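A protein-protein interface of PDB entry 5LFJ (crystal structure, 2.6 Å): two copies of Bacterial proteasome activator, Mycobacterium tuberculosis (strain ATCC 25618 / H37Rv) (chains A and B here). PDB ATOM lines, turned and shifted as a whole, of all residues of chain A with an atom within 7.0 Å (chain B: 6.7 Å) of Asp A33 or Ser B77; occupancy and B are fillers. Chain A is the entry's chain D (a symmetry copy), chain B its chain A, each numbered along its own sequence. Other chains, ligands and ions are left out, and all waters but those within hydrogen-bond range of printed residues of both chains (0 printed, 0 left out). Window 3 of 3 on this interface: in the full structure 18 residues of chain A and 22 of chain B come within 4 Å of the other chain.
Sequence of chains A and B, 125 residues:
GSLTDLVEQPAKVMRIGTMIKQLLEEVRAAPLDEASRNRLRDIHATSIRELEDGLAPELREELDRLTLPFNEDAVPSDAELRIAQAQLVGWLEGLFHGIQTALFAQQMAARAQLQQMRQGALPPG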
ATOM      1  N   PRO A  31      -4.201  19.832 -23.185  1.00  0.00           N
ATOM      2  CA  PRO A  31      -5.100  19.911 -22.019  1.00  0.00           C
ATOM      3  C   PRO A  31      -6.035  18.712 -21.913  1.00  0.00           C
ATOM      4  O   PRO A  31      -6.335  18.025 -22.893  1.00  0.00           O
ATOM      5  CB  PRO A  31      -5.885  21.206 -22.265  1.00  0.00           C
ATOM      6  CG  PRO A  31      -4.986  22.019 -23.146  1.00  0.00           C
ATOM      7  CD  PRO A  31      -4.322  21.020 -24.048  1.00  0.00           C
ATOM      8  N   LEU A  32      -6.504  18.471 -20.689  1.00  0.00           N
ATOM      9  CA  LEU A  32      -7.328  17.318 -20.363  1.00  0.00           C
ATOM     10  C   LEU A  32      -8.709  17.774 -19.907  1.00  0.00           C
ATOM     11  O   LEU A  32      -8.912  18.931 -19.525  1.00  0.00           O
ATOM     12  CB  LEU A  32      -6.687  16.446 -19.267  1.00  0.00           C
ATOM     13  CG  LEU A  32      -5.328  15.793 -19.576  1.00  0.00           C
ATOM     14  CD1 LEU A  32      -4.760  15.024 -18.378  1.00  0.00           C
ATOM     15  CD2 LEU A  32      -5.407  14.878 -20.784  1.00  0.00           C
ATOM     16  N   ASP A  33      -9.661  16.847 -19.967  1.00  0.00           N
ATOM     17  CA  ASP A  33     -11.027  17.077 -19.532  1.00  0.00           C
ATOM     18  C   ASP A  33     -11.288  16.405 -18.181  1.00  0.00           C
ATOM     19  O   ASP A  33     -10.387  15.846 -17.549  1.00  0.00           O
ATOM     20  CB  ASP A  33     -12.017  16.623 -20.615  1.00  0.00           C
ATOM     21  CG  ASP A  33     -11.994  15.127 -20.877  1.00  0.00           C
ATOM     22  OD1 ASP A  33     -11.278  14.376 -20.179  1.00  0.00           O
ATOM     23  OD2 ASP A  33     -12.743  14.695 -21.781  1.00  0.00           O
ATOM     24  N   GLU A  34     -12.547  16.442 -17.748  1.00  0.00           N
ATOM     25  CA  GLU A  34     -12.945  15.910 -16.448  1.00  0.00           C
ATOM     26  C   GLU A  34     -12.593  14.428 -16.307  1.00  0.00           C
ATOM     27  O   GLU A  34     -11.836  14.026 -15.411  1.00  0.00           O
ATOM     28  CB  GLU A  34     -14.461  16.107 -16.312  1.00  0.00           C
ATOM     29  CG  GLU A  34     -15.128  15.744 -14.998  1.00  0.00           C
ATOM     30  CD  GLU A  34     -14.836  16.725 -13.890  1.00  0.00           C
ATOM     31  OE1 GLU A  34     -14.243  17.789 -14.168  1.00  0.00           O
ATOM     32  OE2 GLU A  34     -15.238  16.441 -12.743  1.00  0.00           O
ATOM     33  N   ALA A  35     -13.110  13.607 -17.225  1.00  0.00           N
ATOM     34  CA  ALA A  35     -13.017  12.158 -17.095  1.00  0.00           C
ATOM     35  C   ALA A  35     -11.570  11.682 -17.146  1.00  0.00           C
ATOM     36  O   ALA A  35     -11.161  10.831 -16.348  1.00  0.00           O
ATOM     37  CB  ALA A  35     -13.844  11.491 -18.189  1.00  0.00           C
ATOM     38  N   SER A  36     -10.779  12.233 -18.067  1.00  0.00           N
ATOM     39  CA  SER A  36      -9.393  11.806 -18.204  1.00  0.00           C
ATOM     40  C   SER A  36      -8.550  12.202 -16.989  1.00  0.00           C
ATOM     41  O   SER A  36      -7.656  11.448 -16.576  1.00  0.00           O
ATOM     42  CB  SER A  36      -8.822  12.354 -19.513  1.00  0.00           C
ATOM     43  OG  SER A  36      -8.754  13.759 -19.543  1.00  0.00           O
ATOM     44  N   ARG A  37      -8.839  13.355 -16.374  1.00  0.00           N
ATOM     45  CA  ARG A  37      -8.176  13.705 -15.117  1.00  0.00           C
ATOM     46  C   ARG A  37      -8.568  12.753 -13.996  1.00  0.00           C
ATOM     47  O   ARG A  37      -7.724  12.345 -13.189  1.00  0.00           O
ATOM     48  CB  ARG A  37      -8.494  15.147 -14.717  1.00  0.00           C
ATOM     49  CG  ARG A  37      -7.744  16.195 -15.528  1.00  0.00           C
ATOM     50  CD  ARG A  37      -7.865  17.591 -14.910  1.00  0.00           C
ATOM     51  NE  ARG A  37      -9.246  18.054 -14.878  1.00  0.00           N
ATOM     52  CZ  ARG A  37      -9.828  18.707 -15.876  1.00  0.00           C
ATOM     53  NH1 ARG A  37      -9.146  18.977 -16.992  1.00  0.00           N
ATOM     54  NH2 ARG A  37     -11.092  19.084 -15.757  1.00  0.00           N
ATOM     55  N   ASN A  38      -9.839  12.366 -13.931  1.00  0.00           N
ATOM     56  CA  ASN A  38     -10.229  11.435 -12.881  1.00  0.00           C
ATOM     57  C   ASN A  38      -9.495  10.107 -13.040  1.00  0.00           C
ATOM     58  O   ASN A  38      -8.864   9.609 -12.096  1.00  0.00           O
ATOM     59  CB  ASN A  38     -11.739  11.215 -12.916  1.00  0.00           C
ATOM     60  CG  ASN A  38     -12.264  10.698 -11.608  1.00  0.00           C
ATOM     61  OD1 ASN A  38     -11.859  11.171 -10.546  1.00  0.00           O
ATOM     62  ND2 ASN A  38     -13.119   9.685 -11.664  1.00  0.00           N
ATOM     63  N   VAL A  75     -11.623  16.267  -8.172  1.00  0.00           N
ATOM     64  CA  VAL A  75     -10.860  15.975  -9.393  1.00  0.00           C
ATOM     65  C   VAL A  75      -9.683  16.931  -9.478  1.00  0.00           C
ATOM     66  O   VAL A  75      -9.855  18.145  -9.371  1.00  0.00           O
ATOM     67  CB  VAL A  75     -11.793  16.024 -10.612  1.00  0.00           C
ATOM     68  CG1 VAL A  75     -13.261  16.175 -10.060  1.00  0.00           C
ATOM     69  CG2 VAL A  75     -11.390  17.212 -11.636  1.00  0.00           C
ATOM     70  N   PRO A  76      -8.459  16.412  -9.564  1.00  0.00           N
ATOM     71  CA  PRO A  76      -7.292  17.287  -9.505  1.00  0.00           C
ATOM     72  C   PRO A  76      -7.101  18.033 -10.808  1.00  0.00           C
ATOM     73  O   PRO A  76      -7.527  17.617 -11.885  1.00  0.00           O
ATOM     74  CB  PRO A  76      -6.143  16.304  -9.250  1.00  0.00           C
ATOM     75  CG  PRO A  76      -6.801  15.046  -8.730  1.00  0.00           C
ATOM     76  CD  PRO A  76      -8.098  15.000  -9.462  1.00  0.00           C
ATOM     77  N   ASP A  78      -4.991  19.741 -14.013  1.00  0.00           N
ATOM     78  CA  ASP A  78      -3.847  19.380 -14.847  1.00  0.00           C
ATOM     79  C   ASP A  78      -2.525  19.675 -14.139  1.00  0.00           C
ATOM     80  O   ASP A  78      -1.593  18.852 -14.157  1.00  0.00           O
ATOM     81  CB  ASP A  78      -3.893  20.139 -16.182  1.00  0.00           C
ATOM     82  CG  ASP A  78      -5.031  19.691 -17.093  1.00  0.00           C
ATOM     83  OD1 ASP A  78      -5.640  18.634 -16.833  1.00  0.00           O
ATOM     84  OD2 ASP A  78      -5.308  20.404 -18.087  1.00  0.00           O
ATOM     85  N   VAL B  27      -4.056   9.531 -32.787  1.00  0.00           N
ATOM     86  CA  VAL B  27      -4.931  10.379 -31.987  1.00  0.00           C
ATOM     87  C   VAL B  27      -4.269  11.723 -31.715  1.00  0.00           C
ATOM     88  O   VAL B  27      -4.900  12.779 -31.855  1.00  0.00           O
ATOM     89  CB  VAL B  27      -5.310   9.675 -30.677  1.00  0.00           C
ATOM     90  CG1 VAL B  27      -6.200  10.579 -29.843  1.00  0.00           C
ATOM     91  CG2 VAL B  27      -5.988   8.393 -30.991  1.00  0.00           C
ATOM     92  N   ARG B  37     -13.889   7.569 -32.371  1.00  0.00           N
ATOM     93  CA  ARG B  37     -13.579   7.395 -30.954  1.00  0.00           C
ATOM     94  C   ARG B  37     -14.211   6.121 -30.395  1.00  0.00           C
ATOM     95  O   ARG B  37     -13.619   5.455 -29.535  1.00  0.00           O
ATOM     96  CB  ARG B  37     -14.031   8.614 -30.146  1.00  0.00           C
ATOM     97  CG  ARG B  37     -13.335   9.925 -30.524  1.00  0.00           C
ATOM     98  CD  ARG B  37     -13.545  11.018 -29.466  1.00  0.00           C
ATOM     99  NE  ARG B  37     -14.945  11.366 -29.247  1.00  0.00           N
ATOM    100  CZ  ARG B  37     -15.607  12.280 -29.952  1.00  0.00           C
ATOM    101  NH1 ARG B  37     -14.974  12.927 -30.928  1.00  0.00           N
ATOM    102  NH2 ARG B  37     -16.894  12.547 -29.682  1.00  0.00           N
ATOM    103  N   PHE B  70     -13.235   1.079 -20.377  1.00  0.00           N
ATOM    104  CA  PHE B  70     -14.044   2.258 -20.618  1.00  0.00           C
ATOM    105  C   PHE B  70     -15.513   2.019 -20.315  1.00  0.00           C
ATOM    106  O   PHE B  70     -16.049   0.916 -20.475  1.00  0.00           O
ATOM    107  CB  PHE B  70     -13.921   2.750 -22.058  1.00  0.00           C
ATOM    108  CG  PHE B  70     -12.686   3.524 -22.329  1.00  0.00           C
ATOM    109  CD1 PHE B  70     -12.654   4.880 -22.024  1.00  0.00           C
ATOM    110  CD2 PHE B  70     -11.570   2.933 -22.902  1.00  0.00           C
ATOM    111  CE1 PHE B  70     -11.533   5.634 -22.282  1.00  0.00           C
ATOM    112  CE2 PHE B  70     -10.437   3.677 -23.152  1.00  0.00           C
ATOM    113  CZ  PHE B  70     -10.417   5.036 -22.844  1.00  0.00           C
ATOM    114  N   VAL B  75     -19.143   7.870 -25.083  1.00  0.00           N
ATOM    115  CA  VAL B  75     -18.030   7.837 -26.013  1.00  0.00           C
ATOM    116  C   VAL B  75     -16.901   8.647 -25.362  1.00  0.00           C
ATOM    117  O   VAL B  75     -17.163   9.768 -24.891  1.00  0.00           O
ATOM    118  CB  VAL B  75     -18.397   8.367 -27.411  1.00  0.00           C
ATOM    119  CG1 VAL B  75     -19.832   7.966 -27.762  1.00  0.00           C
ATOM    120  CG2 VAL B  75     -18.150   9.878 -27.589  1.00  0.00           C
ATOM    121  N   PRO B  76     -15.722   8.084 -25.185  1.00  0.00           N
ATOM    122  CA  PRO B  76     -14.680   8.812 -24.466  1.00  0.00           C
ATOM    123  C   PRO B  76     -14.132   9.949 -25.307  1.00  0.00           C
ATOM    124  O   PRO B  76     -14.296  10.000 -26.528  1.00  0.00           O
ATOM    125  CB  PRO B  76     -13.624   7.742 -24.199  1.00  0.00           C
ATOM    126  CG  PRO B  76     -13.861   6.715 -25.268  1.00  0.00           C
ATOM    127  CD  PRO B  76     -15.334   6.689 -25.453  1.00  0.00           C
ATOM    128  N   SER B  77     -13.509  10.897 -24.625  1.00  0.00           N
ATOM    129  CA  SER B  77     -12.938  12.012 -25.352  1.00  0.00           C
ATOM    130  C   SER B  77     -11.580  11.610 -25.909  1.00  0.00           C
ATOM    131  O   SER B  77     -10.986  10.617 -25.480  1.00  0.00           O
ATOM    132  CB  SER B  77     -12.772  13.206 -24.431  1.00  0.00           C
ATOM    133  OG  SER B  77     -11.926  12.850 -23.353  1.00  0.00           O
ATOM    134  N   ASP B  78     -11.079  12.407 -26.860  1.00  0.00           N
ATOM    135  CA  ASP B  78      -9.719  12.201 -27.352  1.00  0.00           C
ATOM    136  C   ASP B  78      -8.721  12.103 -26.202  1.00  0.00           C
ATOM    137  O   ASP B  78      -7.770  11.310 -26.253  1.00  0.00           O
ATOM    138  CB  ASP B  78      -9.287  13.322 -28.306  1.00  0.00           C
ATOM    139  CG  ASP B  78     -10.049  13.320 -29.638  1.00  0.00           C
ATOM    140  OD1 ASP B  78     -10.782  12.350 -29.931  1.00  0.00           O
ATOM    141  OD2 ASP B  78      -9.841  14.265 -30.436  1.00  0.00           O
ATOM    142  N   ALA B  79      -8.914  12.918 -25.164  1.00  0.00           N
ATOM    143  CA  ALA B  79      -7.986  12.921 -24.037  1.00  0.00           C
ATOM    144  C   ALA B  79      -8.009  11.586 -23.304  1.00  0.00           C
ATOM    145  O   ALA B  79      -6.957  11.029 -22.973  1.00  0.00           O
ATOM    146  CB  ALA B  79      -8.325  14.064 -23.080  1.00  0.00           C
ATOM    147  N   GLU B  80      -9.208  11.077 -23.019  1.00  0.00           N
ATOM    148  CA  GLU B  80      -9.366   9.852 -22.246  1.00  0.00           C
ATOM    149  C   GLU B  80      -8.737   8.667 -22.977  1.00  0.00           C
ATOM    150  O   GLU B  80      -8.049   7.828 -22.372  1.00  0.00           O
ATOM    151  CB  GLU B  80     -10.856   9.664 -21.991  1.00  0.00           C
ATOM    152  CG  GLU B  80     -11.289   8.758 -20.874  1.00  0.00           C
ATOM    153  CD  GLU B  80     -12.790   8.911 -20.628  1.00  0.00           C
ATOM    154  OE1 GLU B  80     -13.437   9.737 -21.330  1.00  0.00           O
ATOM    155  OE2 GLU B  80     -13.316   8.219 -19.730  1.00  0.00           O
ATOM    156  N   LEU B  81      -8.964   8.601 -24.288  1.00  0.00           N
ATOM    157  CA  LEU B  81      -8.348   7.595 -25.128  1.00  0.00           C
ATOM    158  C   LEU B  81      -6.831   7.728 -25.091  1.00  0.00           C
ATOM    159  O   LEU B  81      -6.092   6.741 -24.947  1.00  0.00           O
ATOM    160  CB  LEU B  81      -8.869   7.761 -26.553  1.00  0.00           C
ATOM    161  CG  LEU B  81     -10.321   7.411 -26.860  1.00  0.00           C
ATOM    162  CD1 LEU B  81     -10.658   7.834 -28.272  1.00  0.00           C
ATOM    163  CD2 LEU B  81     -10.499   5.911 -26.733  1.00  0.00           C
ATOM    164  N   ARG B  82      -6.355   8.960 -25.192  1.00  0.00           N
ATOM    165  CA  ARG B  82      -4.925   9.206 -25.219  1.00  0.00           C
ATOM    166  C   ARG B  82      -4.275   8.729 -23.915  1.00  0.00           C
ATOM    167  O   ARG B  82      -3.209   8.091 -23.934  1.00  0.00           O
ATOM    168  CB  ARG B  82      -4.730  10.698 -25.496  1.00  0.00           C
ATOM    169  CG  ARG B  82      -3.536  11.094 -26.337  1.00  0.00           C
ATOM    170  CD  ARG B  82      -3.637  12.587 -26.728  1.00  0.00           C
ATOM    171  NE  ARG B  82      -3.480  13.478 -25.581  1.00  0.00           N
ATOM    172  CZ  ARG B  82      -4.323  14.462 -25.281  1.00  0.00           C
ATOM    173  NH1 ARG B  82      -5.379  14.682 -26.051  1.00  0.00           N
ATOM    174  NH2 ARG B  82      -4.113  15.226 -24.215  1.00  0.00           N
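Among the printed residues, merely in contact across the chains: Ser A36 with Ala B79 (3.6 Å), Ala A35 with Glu B80 (3.6 Å), Leu A32 with Arg B82 (3.7 Å), Ser A36 with Glu B80 (3.7 Å), Leu A32 with Ala B79 (3.8 Å) and Pro A31 with Arg B82 (3.8 Å).
Of chain B, only Ser B77 comes within 4 Å of Asp A33.
Ser B77 touches just one residue of chain A: Asp A33 (2.6 Å).
Of the printed residues of chain B, Pro A31 touches Arg B82 (3.8 Å).
Of the printed residues of chain A, Arg B82 touches Pro A31 (3.8 Å) and Leu A32 (3.7 Å).
Of the printed residues of chain B, Ala A35 touches Glu B80.
Of the printed residues of chain A, Glu B80 touches Ala A35 (3.6 Å) and Ser A36 (3.7 Å).
Of the printed residues of chain B, Ser A36 touches Ala B79 (3.6 Å) and Glu B80 (3.7 Å).
Of the 11 printed residues of chain A, 5 touch a printed residue of chain B.
Printed residues of chain A that touch a printed residue of chain B: Pro A31, Leu A32, Asp A33, Ala A35 and Ser A36.
Hydrophobic or aromatic side chains of chain A within 4 Å of the printed part of chain B: Leu A32 and Ala A35.
Of the 11 printed residues of chain B, 4 touch a printed residue of chain A.
Hydrophobic or aromatic side chains of chain B within 4 Å of the printed part of chain A: Ala B79.
Among the printed residues, 7 pairs touch across the chains.
Among the printed residues, no Asp or Glu carboxylate lies within 4 Å of a Lys or Arg side-chain nitrogen of the other chain.
The side-chain carboxylate of Asp A33 lies within hydrogen-bond range of the side-chain hydroxyl of Ser B77, at 2.6 Å.
4 positions are printed for both chains.
Of the 7 pairs that touch across the chains among the printed residues, none has its exchanged pair printed and touching as well.
NH1 of Arg A37 lies close to O of Asp A33, 3.4 Å away.
The side-chain carboxylate (OD2) of Asp A78 lies within hydrogen-bond range of the backbone NH (N) of Leu A32.
The side-chain carboxylate (OD1) of Asp A33 sits at hydrogen-bond distance from the side-chain hydroxyl (OG) of Ser A36 (2.7 Å).
The guanidinium group (NH1) of Arg A37 is in hydrogen-bond range of the backbone carbonyl oxygen (O) of Leu A32.
The backbone NH (N) of Glu B80 is in hydrogen-bond range of the side-chain hydroxyl (OG) of Ser B77 (3.3 Å).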
